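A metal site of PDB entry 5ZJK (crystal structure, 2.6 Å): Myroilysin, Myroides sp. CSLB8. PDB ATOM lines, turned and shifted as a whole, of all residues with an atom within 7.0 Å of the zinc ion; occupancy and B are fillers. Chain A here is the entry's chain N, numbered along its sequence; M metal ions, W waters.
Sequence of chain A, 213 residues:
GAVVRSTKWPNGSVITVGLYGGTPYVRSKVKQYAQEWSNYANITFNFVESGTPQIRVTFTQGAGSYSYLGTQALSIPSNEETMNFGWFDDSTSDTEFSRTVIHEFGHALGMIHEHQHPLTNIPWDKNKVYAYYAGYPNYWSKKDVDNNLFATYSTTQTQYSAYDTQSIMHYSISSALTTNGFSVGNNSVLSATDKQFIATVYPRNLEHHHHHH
O of Ile 168 lies within hydrogen-bond range of ND1 of His 103, at 2.7 Å. A ring nitrogen (ND1) of His 107 lies within hydrogen-bond range of the backbone carbonyl oxygen (O) of Met 111 (2.9 Å).
Of the 13 residues printed, 4 come within 4 Å of the zinc ion.
The zinc ion is bound by water W1 (2.2 Å), NE2 of His 103 (2.2 Å), NE2 of His 107 (2.2 Å), NE2 of His 113 (2.3 Å) and OH of Tyr 171 (2.3 Å).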
ATOM      1  N   SER A  65     -11.676   0.918   3.039  1.00  0.00           N
ATOM      2  CA  SER A  65     -12.826   1.680   3.489  1.00  0.00           C
ATOM      3  C   SER A  65     -12.389   2.990   4.152  1.00  0.00           C
ATOM      4  O   SER A  65     -11.804   2.981   5.231  1.00  0.00           O
ATOM      5  CB  SER A  65     -13.689   0.866   4.446  1.00  0.00           C
ATOM      6  OG  SER A  65     -14.375  -0.166   3.766  1.00  0.00           O
ATOM      7  N   TYR A  66     -12.677   4.100   3.484  1.00  0.00           N
ATOM      8  CA  TYR A  66     -12.245   5.409   3.950  1.00  0.00           C
ATOM      9  C   TYR A  66     -13.290   6.465   3.644  1.00  0.00           C
ATOM     10  O   TYR A  66     -13.817   6.521   2.529  1.00  0.00           O
ATOM     11  CB  TYR A  66     -10.901   5.784   3.300  1.00  0.00           C
ATOM     12  CG  TYR A  66     -10.964   5.896   1.793  1.00  0.00           C
ATOM     13  CD1 TYR A  66     -10.899   4.762   0.985  1.00  0.00           C
ATOM     14  CD2 TYR A  66     -11.095   7.135   1.181  1.00  0.00           C
ATOM     15  CE1 TYR A  66     -10.963   4.871  -0.391  1.00  0.00           C
ATOM     16  CE2 TYR A  66     -11.166   7.246  -0.202  1.00  0.00           C
ATOM     17  CZ  TYR A  66     -11.089   6.105  -0.979  1.00  0.00           C
ATOM     18  OH  TYR A  66     -11.158   6.221  -2.350  1.00  0.00           O
ATOM     19  N   SER A  67     -13.600   7.303   4.625  1.00  0.00           N
ATOM     20  CA  SER A  67     -14.498   8.422   4.414  1.00  0.00           C
ATOM     21  C   SER A  67     -13.947   9.661   5.090  1.00  0.00           C
ATOM     22  O   SER A  67     -13.355   9.586   6.176  1.00  0.00           O
ATOM     23  CB  SER A  67     -15.901   8.116   4.935  1.00  0.00           C
ATOM     24  OG  SER A  67     -16.706   9.292   4.947  1.00  0.00           O
ATOM     25  N   HIS A 103     -20.255   2.702  10.227  1.00  0.00           N
ATOM     26  CA  HIS A 103     -19.035   3.193  10.778  1.00  0.00           C
ATOM     27  C   HIS A 103     -18.421   4.213   9.844  1.00  0.00           C
ATOM     28  O   HIS A 103     -17.789   5.138  10.252  1.00  0.00           O
ATOM     29  CB  HIS A 103     -18.098   2.016  10.979  1.00  0.00           C
ATOM     30  CG  HIS A 103     -16.717   2.404  11.354  1.00  0.00           C
ATOM     31  ND1 HIS A 103     -16.129   1.978  12.514  1.00  0.00           N
ATOM     32  CD2 HIS A 103     -15.797   3.165  10.718  1.00  0.00           C
ATOM     33  CE1 HIS A 103     -14.917   2.483  12.596  1.00  0.00           C
ATOM     34  NE2 HIS A 103     -14.685   3.202  11.527  1.00  0.00           N
ATOM     35  N   GLU A 104     -18.626   4.036   8.565  1.00  0.00           N
ATOM     36  CA  GLU A 104     -18.046   4.963   7.633  1.00  0.00           C
ATOM     37  C   GLU A 104     -18.930   6.193   7.563  1.00  0.00           C
ATOM     38  O   GLU A 104     -18.482   7.275   7.308  1.00  0.00           O
ATOM     39  CB  GLU A 104     -17.807   4.296   6.283  1.00  0.00           C
ATOM     40  CG  GLU A 104     -16.416   4.500   5.694  1.00  0.00           C
ATOM     41  CD  GLU A 104     -15.248   4.234   6.655  1.00  0.00           C
ATOM     42  OE1 GLU A 104     -15.261   3.225   7.378  1.00  0.00           O
ATOM     43  OE2 GLU A 104     -14.298   5.016   6.646  1.00  0.00           O
ATOM     44  N   HIS A 107     -18.048   8.417  10.187  1.00  0.00           N
ATOM     45  CA  HIS A 107     -17.026   9.332   9.828  1.00  0.00           C
ATOM     46  C   HIS A 107     -17.701  10.424   9.092  1.00  0.00           C
ATOM     47  O   HIS A 107     -17.414  11.569   9.307  1.00  0.00           O
ATOM     48  CB  HIS A 107     -16.051   8.673   8.885  1.00  0.00           C
ATOM     49  CG  HIS A 107     -15.020   7.864   9.577  1.00  0.00           C
ATOM     50  ND1 HIS A 107     -14.186   8.380  10.530  1.00  0.00           N
ATOM     51  CD2 HIS A 107     -14.683   6.568   9.441  1.00  0.00           C
ATOM     52  CE1 HIS A 107     -13.383   7.432  10.963  1.00  0.00           C
ATOM     53  NE2 HIS A 107     -13.665   6.323  10.314  1.00  0.00           N
ATOM     54  N   MET A 111     -17.469  11.741  13.103  1.00  0.00           N
ATOM     55  CA  MET A 111     -16.871  10.974  14.193  1.00  0.00           C
ATOM     56  C   MET A 111     -15.498  10.444  13.810  1.00  0.00           C
ATOM     57  O   MET A 111     -15.251  10.077  12.664  1.00  0.00           O
ATOM     58  CB  MET A 111     -17.773   9.808  14.606  1.00  0.00           C
ATOM     59  CG  MET A 111     -19.134  10.227  15.126  1.00  0.00           C
ATOM     60  SD  MET A 111     -19.949   8.912  16.057  1.00  0.00           S
ATOM     61  CE  MET A 111     -18.936   8.868  17.529  1.00  0.00           C
ATOM     62  N   ILE A 112     -14.602  10.422  14.786  1.00  0.00           N
ATOM     63  CA  ILE A 112     -13.254   9.894  14.589  1.00  0.00           C
ATOM     64  C   ILE A 112     -13.177   8.459  15.068  1.00  0.00           C
ATOM     65  O   ILE A 112     -14.154   7.895  15.544  1.00  0.00           O
ATOM     66  CB  ILE A 112     -12.220  10.741  15.349  1.00  0.00           C
ATOM     67  CG1 ILE A 112     -12.614  10.831  16.820  1.00  0.00           C
ATOM     68  CG2 ILE A 112     -12.115  12.121  14.743  1.00  0.00           C
ATOM     69  CD1 ILE A 112     -11.511  11.266  17.739  1.00  0.00           C
ATOM     70  N   HIS A 113     -11.976   7.886  15.028  1.00  0.00           N
ATOM     71  CA  HIS A 113     -11.764   6.524  15.471  1.00  0.00           C
ATOM     72  C   HIS A 113     -11.683   6.556  16.977  1.00  0.00           C
ATOM     73  O   HIS A 113     -10.963   7.346  17.555  1.00  0.00           O
ATOM     74  CB  HIS A 113     -10.500   5.937  14.870  1.00  0.00           C
ATOM     75  CG  HIS A 113     -10.576   5.748  13.396  1.00  0.00           C
ATOM     76  ND1 HIS A 113      -9.892   6.568  12.522  1.00  0.00           N
ATOM     77  CD2 HIS A 113     -11.295   4.906  12.632  1.00  0.00           C
ATOM     78  CE1 HIS A 113     -10.171   6.205  11.293  1.00  0.00           C
ATOM     79  NE2 HIS A 113     -10.997   5.175  11.339  1.00  0.00           N
ATOM     80  N   HIS A 115     -10.274   4.722  19.075  1.00  0.00           N
ATOM     81  CA  HIS A 115      -8.961   4.477  19.659  1.00  0.00           C
ATOM     82  C   HIS A 115      -8.104   5.732  19.558  1.00  0.00           C
ATOM     83  O   HIS A 115      -7.012   5.808  20.120  1.00  0.00           O
ATOM     84  CB  HIS A 115      -8.264   3.298  18.975  1.00  0.00           C
ATOM     85  CG  HIS A 115      -7.860   3.565  17.557  1.00  0.00           C
ATOM     86  ND1 HIS A 115      -8.674   3.263  16.485  1.00  0.00           N
ATOM     87  CD2 HIS A 115      -6.726   4.095  17.042  1.00  0.00           C
ATOM     88  CE1 HIS A 115      -8.052   3.604  15.368  1.00  0.00           C
ATOM     89  NE2 HIS A 115      -6.876   4.112  15.676  1.00  0.00           N
ATOM     90  N   ILE A 168     -19.200   2.133  17.946  1.00  0.00           N
ATOM     91  CA  ILE A 168     -19.188   1.735  16.540  1.00  0.00           C
ATOM     92  C   ILE A 168     -17.945   2.260  15.840  1.00  0.00           C
ATOM     93  O   ILE A 168     -17.527   1.737  14.802  1.00  0.00           O
ATOM     94  CB  ILE A 168     -20.446   2.245  15.797  1.00  0.00           C
ATOM     95  CG1 ILE A 168     -20.734   1.411  14.549  1.00  0.00           C
ATOM     96  CG2 ILE A 168     -20.303   3.732  15.466  1.00  0.00           C
ATOM     97  CD1 ILE A 168     -20.645  -0.092  14.768  1.00  0.00           C
ATOM     98  N   MET A 169     -17.302   3.234  16.449  1.00  0.00           N
ATOM     99  CA  MET A 169     -16.131   3.788  15.872  1.00  0.00           C
ATOM    100  C   MET A 169     -14.920   3.182  16.483  1.00  0.00           C
ATOM    101  O   MET A 169     -13.889   3.768  16.507  1.00  0.00           O
ATOM    102  CB  MET A 169     -16.128   5.244  16.172  1.00  0.00           C
ATOM    103  CG  MET A 169     -17.462   5.829  15.858  1.00  0.00           C
ATOM    104  SD  MET A 169     -17.789   5.546  14.159  1.00  0.00           S
ATOM    105  CE  MET A 169     -16.557   6.526  13.365  1.00  0.00           C
ATOM    106  N   TYR A 171     -12.407  -0.211  16.596  1.00  0.00           N
ATOM    107  CA  TYR A 171     -12.016  -1.474  16.035  1.00  0.00           C
ATOM    108  C   TYR A 171     -11.601  -2.458  17.091  1.00  0.00           C
ATOM    109  O   TYR A 171     -11.693  -2.221  18.211  1.00  0.00           O
ATOM    110  CB  TYR A 171     -10.888  -1.277  15.061  1.00  0.00           C
ATOM    111  CG  TYR A 171     -11.232  -0.386  13.912  1.00  0.00           C
ATOM    112  CD1 TYR A 171     -12.257  -0.710  13.038  1.00  0.00           C
ATOM    113  CD2 TYR A 171     -10.537   0.752  13.691  1.00  0.00           C
ATOM    114  CE1 TYR A 171     -12.567   0.112  11.983  1.00  0.00           C
ATOM    115  CE2 TYR A 171     -10.841   1.559  12.640  1.00  0.00           C
ATOM    116  CZ  TYR A 171     -11.861   1.245  11.792  1.00  0.00           C
ATOM    117  OH  TYR A 171     -12.173   2.092  10.759  1.00  0.00           O
HETATM  118 ZN    ZN M   1     -12.912   4.223  10.606  1.00  0.00          ZN
HETATM  119  O   HOH W   1     -12.153   4.552   8.546  1.00  0.00           O
